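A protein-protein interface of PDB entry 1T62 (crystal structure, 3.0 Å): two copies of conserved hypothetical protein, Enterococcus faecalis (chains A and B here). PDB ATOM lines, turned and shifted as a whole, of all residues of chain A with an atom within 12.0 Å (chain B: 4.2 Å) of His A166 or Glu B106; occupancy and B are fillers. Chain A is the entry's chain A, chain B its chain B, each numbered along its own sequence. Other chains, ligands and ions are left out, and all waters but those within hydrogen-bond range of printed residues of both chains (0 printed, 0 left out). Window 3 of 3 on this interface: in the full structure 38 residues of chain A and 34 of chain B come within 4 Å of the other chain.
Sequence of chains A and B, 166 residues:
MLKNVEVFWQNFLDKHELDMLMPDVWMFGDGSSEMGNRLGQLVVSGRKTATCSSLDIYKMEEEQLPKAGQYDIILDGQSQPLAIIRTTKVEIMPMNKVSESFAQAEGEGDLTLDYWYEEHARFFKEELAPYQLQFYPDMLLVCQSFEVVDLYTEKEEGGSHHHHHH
The backbone carbonyl oxygen (O) of Ala B50 is in hydrogen-bond range of the side-chain amino group (NZ) of Lys B48. OE2 of Glu B106 lies within salt-bridge range of NZ of Lys B48 (3.3 Å). The side-chain carboxylate (OE1) of Glu B106 is in hydrogen-bond range of the side-chain sulfur (SG) of Cys B52, at 3.1 Å. The side-chain sulfur (SG) of Cys B52 lies close to a ring nitrogen (NE2) of His B120 (3.8 Å). OE1 of Glu B106 is in hydrogen-bond range of NE2 of His B120, 3.0 Å away. ND1 of His B120 is in hydrogen-bond range of O of Trp B116, at 2.8 Å.
The chain-end carboxylate of His A166 is in salt-bridge range of the side-chain amino group of Lys B48 (2.7 Å). The backbone carbonyl oxygen (O) of Cys B52 lies within hydrogen-bond range of the backbone NH (N) of His A166 (3.2 Å). The side-chain carboxylate of Glu B106 is in hydrogen-bond range of a ring nitrogen (ND1) of His A166, at 3.4 Å. A ring nitrogen (ND1) of His A166 is in hydrogen-bond range of a ring nitrogen (NE2) of His B120 (3.3 Å).
Of the 15 printed residues of chain B, 8 touch a printed residue of chain A. Along chain B the printed residues that touch a printed residue of chain A span positions 28 to 123. Of the 5 printed residues of chain A, 3 touch a printed residue of chain B. Hydrophobic or aromatic side chains of chain A that line the printed part of chain B: His A164, His A165 and His A166. Among the printed residues, no Asp or Glu carboxylate lies within 4 Å of a Lys or Arg side-chain nitrogen of the other chain.
Of the printed residues of chain B, His A164 touches Cys B52 (3.8 Å) and Phe B123 (3.5 Å). Of the printed residues of chain B, His A165 touches Phe B28 (3.6 Å), Thr B51 (3.2 Å) and Cys B52 (3.9 Å). Of chain B, only Phe B28, Lys B48, Thr B51, Cys B52, Glu B106, Glu B119, His B120 and Phe B123 come within 4 Å of His A166. Of chain A, only His A165 and His A166 come within 4 Å of Phe B28. Lys B48 touches just one residue of chain A: His A166 (2.7 Å). Thr B51 touches two residues of chain A. Of chain A, only His A164 (3.8 Å), His A165 (3.9 Å) and His A166 (3.2 Å) come within 4 Å of Cys B52. No residue of chain A comes within 4 Å of Phe B102. No residue of chain A comes within 4 Å of Ala B105. Printed residues of chain A within 4 Å of Glu B106: His A166. No residue of chain A comes within 4 Å of Gly B107. Trp B116 touches none of the printed residues of chain A. Glu B119 touches just one residue of chain A: His A166. His B120 touches one residue of chain A. The nearest printed residue of chain B that does not touch His A166 is Ala B50 (4.3 Å). The nearest residue of chain A that does not touch Glu B106 is His A165 (6.3 Å).
Among the printed residues, merely in contact across the chains: His A164 with Cys B52 (3.8 Å), His A164 with Phe B123 (3.5 Å), His A165 with Phe B28 (3.6 Å), His A165 with Thr B51 (3.2 Å), His A165 with Cys B52 (3.9 Å), His A166 with Phe B28 (3.2 Å), His A166 with Thr B51 (2.9 Å), His A166 with Glu B119 (3.8 Å) and His A166 with Phe B123 (3.7 Å).
No position is printed for both chains. Of the 13 pairs that touch across the chains among the printed residues, none has its exchanged pair printed and touching as well.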
ATOM      1  N   HIS A 162      -6.127  12.469  -3.945  1.00  0.00           N
ATOM      2  CA  HIS A 162      -5.932  12.820  -2.542  1.00  0.00           C
ATOM      3  C   HIS A 162      -6.469  14.237  -2.323  1.00  0.00           C
ATOM      4  O   HIS A 162      -6.114  15.150  -3.075  1.00  0.00           O
ATOM      5  CB  HIS A 162      -4.440  12.749  -2.204  1.00  0.00           C
ATOM      6  CG  HIS A 162      -4.141  12.870  -0.744  1.00  0.00           C
ATOM      7  ND1 HIS A 162      -4.478  13.985  -0.004  1.00  0.00           N
ATOM      8  CD2 HIS A 162      -3.534  12.019   0.115  1.00  0.00           C
ATOM      9  CE1 HIS A 162      -4.090  13.813   1.247  1.00  0.00           C
ATOM     10  NE2 HIS A 162      -3.514  12.628   1.346  1.00  0.00           N
ATOM     11  N   HIS A 163      -7.308  14.418  -1.298  1.00  0.00           N
ATOM     12  CA  HIS A 163      -7.923  15.727  -1.011  1.00  0.00           C
ATOM     13  C   HIS A 163      -7.301  16.671   0.030  1.00  0.00           C
ATOM     14  O   HIS A 163      -6.458  16.280   0.841  1.00  0.00           O
ATOM     15  CB  HIS A 163      -9.391  15.542  -0.630  1.00  0.00           C
ATOM     16  CG  HIS A 163     -10.273  15.165  -1.776  1.00  0.00           C
ATOM     17  ND1 HIS A 163     -10.380  13.873  -2.245  1.00  0.00           N
ATOM     18  CD2 HIS A 163     -11.092  15.917  -2.548  1.00  0.00           C
ATOM     19  CE1 HIS A 163     -11.231  13.847  -3.255  1.00  0.00           C
ATOM     20  NE2 HIS A 163     -11.678  15.073  -3.459  1.00  0.00           N
ATOM     21  N   HIS A 164      -7.757  17.924  -0.014  1.00  0.00           N
ATOM     22  CA  HIS A 164      -7.322  18.986   0.893  1.00  0.00           C
ATOM     23  C   HIS A 164      -8.535  19.792   1.334  1.00  0.00           C
ATOM     24  O   HIS A 164      -9.193  20.433   0.510  1.00  0.00           O
ATOM     25  CB  HIS A 164      -6.360  19.953   0.207  1.00  0.00           C
ATOM     26  CG  HIS A 164      -4.967  19.435   0.063  1.00  0.00           C
ATOM     27  ND1 HIS A 164      -3.947  20.197  -0.467  1.00  0.00           N
ATOM     28  CD2 HIS A 164      -4.421  18.234   0.368  1.00  0.00           C
ATOM     29  CE1 HIS A 164      -2.833  19.487  -0.481  1.00  0.00           C
ATOM     30  NE2 HIS A 164      -3.094  18.293   0.019  1.00  0.00           N
ATOM     31  N   HIS A 165      -8.829  19.765   2.629  1.00  0.00           N
ATOM     32  CA  HIS A 165      -9.957  20.515   3.148  1.00  0.00           C
ATOM     33  C   HIS A 165      -9.420  21.722   3.894  1.00  0.00           C
ATOM     34  O   HIS A 165      -8.576  21.580   4.778  1.00  0.00           O
ATOM     35  CB  HIS A 165     -10.781  19.676   4.128  1.00  0.00           C
ATOM     36  CG  HIS A 165     -11.158  18.330   3.612  1.00  0.00           C
ATOM     37  ND1 HIS A 165     -10.311  17.245   3.682  1.00  0.00           N
ATOM     38  CD2 HIS A 165     -12.296  17.885   3.034  1.00  0.00           C
ATOM     39  CE1 HIS A 165     -10.914  16.186   3.170  1.00  0.00           C
ATOM     40  NE2 HIS A 165     -12.121  16.548   2.770  1.00  0.00           N
ATOM     41  N   HIS A 166      -9.897  22.910   3.545  1.00  0.00           N
ATOM     42  CA  HIS A 166      -9.453  24.098   4.248  1.00  0.00           C
ATOM     43  C   HIS A 166     -10.577  24.530   5.187  1.00  0.00           C
ATOM     44  O   HIS A 166     -11.043  25.680   5.079  1.00  0.00           O
ATOM     45  CB  HIS A 166      -9.118  25.225   3.270  1.00  0.00           C
ATOM     46  CG  HIS A 166      -8.396  26.373   3.906  1.00  0.00           C
ATOM     47  ND1 HIS A 166      -8.925  27.098   4.954  1.00  0.00           N
ATOM     48  CD2 HIS A 166      -7.173  26.903   3.662  1.00  0.00           C
ATOM     49  CE1 HIS A 166      -8.060  28.024   5.328  1.00  0.00           C
ATOM     50  NE2 HIS A 166      -6.989  27.927   4.560  1.00  0.00           N
ATOM     51  OXT HIS A 166     -10.985  23.704   6.026  1.00  0.00           O
ATOM     52  N   PHE B  28      -7.265  18.653   8.616  1.00  0.00           N
ATOM     53  CA  PHE B  28      -7.517  19.838   7.805  1.00  0.00           C
ATOM     54  C   PHE B  28      -6.220  20.407   7.291  1.00  0.00           C
ATOM     55  O   PHE B  28      -5.196  20.334   7.963  1.00  0.00           O
ATOM     56  CB  PHE B  28      -8.218  20.906   8.625  1.00  0.00           C
ATOM     57  CG  PHE B  28      -9.672  20.659   8.828  1.00  0.00           C
ATOM     58  CD1 PHE B  28     -10.599  21.141   7.925  1.00  0.00           C
ATOM     59  CD2 PHE B  28     -10.124  19.983   9.953  1.00  0.00           C
ATOM     60  CE1 PHE B  28     -11.961  20.964   8.147  1.00  0.00           C
ATOM     61  CE2 PHE B  28     -11.482  19.796  10.190  1.00  0.00           C
ATOM     62  CZ  PHE B  28     -12.408  20.288   9.289  1.00  0.00           C
ATOM     63  N   LYS B  48     -14.722  27.199  13.890  1.00  0.00           N
ATOM     64  CA  LYS B  48     -14.749  26.881  12.462  1.00  0.00           C
ATOM     65  C   LYS B  48     -15.729  25.741  12.194  1.00  0.00           C
ATOM     66  O   LYS B  48     -15.471  24.583  12.540  1.00  0.00           O
ATOM     67  CB  LYS B  48     -13.353  26.495  11.968  1.00  0.00           C
ATOM     68  CG  LYS B  48     -13.337  25.812  10.595  1.00  0.00           C
ATOM     69  CD  LYS B  48     -11.963  25.220  10.325  1.00  0.00           C
ATOM     70  CE  LYS B  48     -11.898  24.475   9.007  1.00  0.00           C
ATOM     71  NZ  LYS B  48     -11.955  25.394   7.832  1.00  0.00           N
ATOM     72  N   ALA B  50     -17.146  25.184   8.978  1.00  0.00           N
ATOM     73  CA  ALA B  50     -17.233  24.941   7.541  1.00  0.00           C
ATOM     74  C   ALA B  50     -15.866  24.664   6.922  1.00  0.00           C
ATOM     75  O   ALA B  50     -14.824  24.985   7.498  1.00  0.00           O
ATOM     76  CB  ALA B  50     -17.873  26.117   6.849  1.00  0.00           C
ATOM     77  N   THR B  51     -15.894  24.077   5.730  1.00  0.00           N
ATOM     78  CA  THR B  51     -14.698  23.719   4.983  1.00  0.00           C
ATOM     79  C   THR B  51     -14.981  23.859   3.502  1.00  0.00           C
ATOM     80  O   THR B  51     -16.113  24.091   3.076  1.00  0.00           O
ATOM     81  CB  THR B  51     -14.334  22.260   5.210  1.00  0.00           C
ATOM     82  OG1 THR B  51     -14.476  21.958   6.597  1.00  0.00           O
ATOM     83  CG2 THR B  51     -12.914  21.992   4.788  1.00  0.00           C
ATOM     84  N   CYS B  52     -13.941  23.700   2.707  1.00  0.00           N
ATOM     85  CA  CYS B  52     -14.115  23.770   1.280  1.00  0.00           C
ATOM     86  C   CYS B  52     -12.951  23.071   0.617  1.00  0.00           C
ATOM     87  O   CYS B  52     -11.801  23.191   1.049  1.00  0.00           O
ATOM     88  CB  CYS B  52     -14.226  25.223   0.815  1.00  0.00           C
ATOM     89  SG  CYS B  52     -12.805  26.234   1.161  1.00  0.00           S
ATOM     90  N   PHE B 102     -20.058  32.595   4.665  1.00  0.00           N
ATOM     91  CA  PHE B 102     -19.339  31.342   4.617  1.00  0.00           C
ATOM     92  C   PHE B 102     -17.923  31.489   5.175  1.00  0.00           C
ATOM     93  O   PHE B 102     -17.406  30.562   5.802  1.00  0.00           O
ATOM     94  CB  PHE B 102     -19.299  30.809   3.173  1.00  0.00           C
ATOM     95  CG  PHE B 102     -18.492  29.541   3.003  1.00  0.00           C
ATOM     96  CD1 PHE B 102     -17.117  29.593   2.765  1.00  0.00           C
ATOM     97  CD2 PHE B 102     -19.097  28.299   3.108  1.00  0.00           C
ATOM     98  CE1 PHE B 102     -16.356  28.420   2.635  1.00  0.00           C
ATOM     99  CE2 PHE B 102     -18.343  27.119   2.981  1.00  0.00           C
ATOM    100  CZ  PHE B 102     -16.967  27.184   2.745  1.00  0.00           C
ATOM    101  N   ALA B 103     -17.298  32.645   4.965  1.00  0.00           N
ATOM    102  CA  ALA B 103     -15.938  32.838   5.445  1.00  0.00           C
ATOM    103  C   ALA B 103     -15.837  32.859   6.967  1.00  0.00           C
ATOM    104  O   ALA B 103     -14.869  32.350   7.528  1.00  0.00           O
ATOM    105  CB  ALA B 103     -15.359  34.098   4.868  1.00  0.00           C
ATOM    106  N   GLN B 104     -16.823  33.439   7.640  1.00  0.00           N
ATOM    107  CA  GLN B 104     -16.794  33.488   9.097  1.00  0.00           C
ATOM    108  C   GLN B 104     -16.999  32.068   9.630  1.00  0.00           C
ATOM    109  O   GLN B 104     -16.355  31.640  10.603  1.00  0.00           O
ATOM    110  CB  GLN B 104     -17.875  34.447   9.616  1.00  0.00           C
ATOM    111  CG  GLN B 104     -17.753  35.852   9.017  1.00  0.00           C
ATOM    112  CD  GLN B 104     -18.682  36.868   9.658  1.00  0.00           C
ATOM    113  OE1 GLN B 104     -19.844  36.572   9.951  1.00  0.00           O
ATOM    114  NE2 GLN B 104     -18.178  38.083   9.861  1.00  0.00           N
ATOM    115  N   ALA B 105     -17.891  31.338   8.972  1.00  0.00           N
ATOM    116  CA  ALA B 105     -18.156  29.959   9.338  1.00  0.00           C
ATOM    117  C   ALA B 105     -16.865  29.158   9.150  1.00  0.00           C
ATOM    118  O   ALA B 105     -16.566  28.250   9.927  1.00  0.00           O
ATOM    119  CB  ALA B 105     -19.232  29.403   8.456  1.00  0.00           C
ATOM    120  N   GLU B 106     -16.108  29.527   8.112  1.00  0.00           N
ATOM    121  CA  GLU B 106     -14.840  28.897   7.724  1.00  0.00           C
ATOM    122  C   GLU B 106     -13.726  29.073   8.749  1.00  0.00           C
ATOM    123  O   GLU B 106     -12.715  28.353   8.707  1.00  0.00           O
ATOM    124  CB  GLU B 106     -14.386  29.479   6.390  1.00  0.00           C
ATOM    125  CG  GLU B 106     -14.290  28.480   5.266  1.00  0.00           C
ATOM    126  CD  GLU B 106     -12.905  27.885   5.121  1.00  0.00           C
ATOM    127  OE1 GLU B 106     -12.684  27.144   4.141  1.00  0.00           O
ATOM    128  OE2 GLU B 106     -12.036  28.152   5.981  1.00  0.00           O
ATOM    129  N   GLY B 107     -13.909  30.038   9.654  1.00  0.00           N
ATOM    130  CA  GLY B 107     -12.915  30.306  10.684  1.00  0.00           C
ATOM    131  C   GLY B 107     -12.542  31.771  10.818  1.00  0.00           C
ATOM    132  O   GLY B 107     -11.666  32.129  11.608  1.00  0.00           O
ATOM    133  N   TRP B 116      -9.316  36.308   2.804  1.00  0.00           N
ATOM    134  CA  TRP B 116      -9.871  34.965   2.832  1.00  0.00           C
ATOM    135  C   TRP B 116      -9.607  34.348   1.472  1.00  0.00           C
ATOM    136  O   TRP B 116      -9.135  33.206   1.352  1.00  0.00           O
ATOM    137  CB  TRP B 116     -11.379  35.018   3.079  1.00  0.00           C
ATOM    138  CG  TRP B 116     -12.019  33.667   3.175  1.00  0.00           C
ATOM    139  CD1 TRP B 116     -12.305  32.972   4.317  1.00  0.00           C
ATOM    140  CD2 TRP B 116     -12.401  32.822   2.085  1.00  0.00           C
ATOM    141  NE1 TRP B 116     -12.838  31.744   4.003  1.00  0.00           N
ATOM    142  CE2 TRP B 116     -12.908  31.626   2.640  1.00  0.00           C
ATOM    143  CE3 TRP B 116     -12.364  32.961   0.691  1.00  0.00           C
ATOM    144  CZ2 TRP B 116     -13.372  30.573   1.850  1.00  0.00           C
ATOM    145  CZ3 TRP B 116     -12.826  31.917  -0.095  1.00  0.00           C
ATOM    146  CH2 TRP B 116     -13.324  30.735   0.490  1.00  0.00           C
ATOM    147  N   GLU B 119      -5.824  33.753   0.747  1.00  0.00           N
ATOM    148  CA  GLU B 119      -5.432  32.573   1.504  1.00  0.00           C
ATOM    149  C   GLU B 119      -5.776  31.301   0.728  1.00  0.00           C
ATOM    150  O   GLU B 119      -4.896  30.509   0.398  1.00  0.00           O
ATOM    151  CB  GLU B 119      -6.138  32.575   2.865  1.00  0.00           C
ATOM    152  CG  GLU B 119      -5.800  31.397   3.771  1.00  0.00           C
ATOM    153  CD  GLU B 119      -6.343  31.575   5.187  1.00  0.00           C
ATOM    154  OE1 GLU B 119      -7.543  31.890   5.331  1.00  0.00           O
ATOM    155  OE2 GLU B 119      -5.574  31.397   6.159  1.00  0.00           O
ATOM    156  N   HIS B 120      -7.053  31.122   0.415  1.00  0.00           N
ATOM    157  CA  HIS B 120      -7.495  29.935  -0.298  1.00  0.00           C
ATOM    158  C   HIS B 120      -6.942  29.798  -1.716  1.00  0.00           C
ATOM    159  O   HIS B 120      -6.703  28.685  -2.198  1.00  0.00           O
ATOM    160  CB  HIS B 120      -9.025  29.888  -0.321  1.00  0.00           C
ATOM    161  CG  HIS B 120      -9.635  29.626   1.021  1.00  0.00           C
ATOM    162  ND1 HIS B 120      -9.483  30.485   2.090  1.00  0.00           N
ATOM    163  CD2 HIS B 120     -10.380  28.591   1.474  1.00  0.00           C
ATOM    164  CE1 HIS B 120     -10.108  29.990   3.144  1.00  0.00           C
ATOM    165  NE2 HIS B 120     -10.661  28.841   2.796  1.00  0.00           N
ATOM    166  N   PHE B 123      -3.720  28.074  -1.195  1.00  0.00           N
ATOM    167  CA  PHE B 123      -3.960  26.714  -0.749  1.00  0.00           C
ATOM    168  C   PHE B 123      -4.295  25.792  -1.920  1.00  0.00           C
ATOM    169  O   PHE B 123      -3.641  24.770  -2.123  1.00  0.00           O
ATOM    170  CB  PHE B 123      -5.110  26.695   0.260  1.00  0.00           C
ATOM    171  CG  PHE B 123      -5.318  25.360   0.909  1.00  0.00           C
ATOM    172  CD1 PHE B 123      -4.418  24.886   1.858  1.00  0.00           C
ATOM    173  CD2 PHE B 123      -6.402  24.560   0.555  1.00  0.00           C
ATOM    174  CE1 PHE B 123      -4.590  23.637   2.447  1.00  0.00           C
ATOM    175  CE2 PHE B 123      -6.583  23.305   1.138  1.00  0.00           C
ATOM    176  CZ  PHE B 123      -5.673  22.844   2.087  1.00  0.00           C
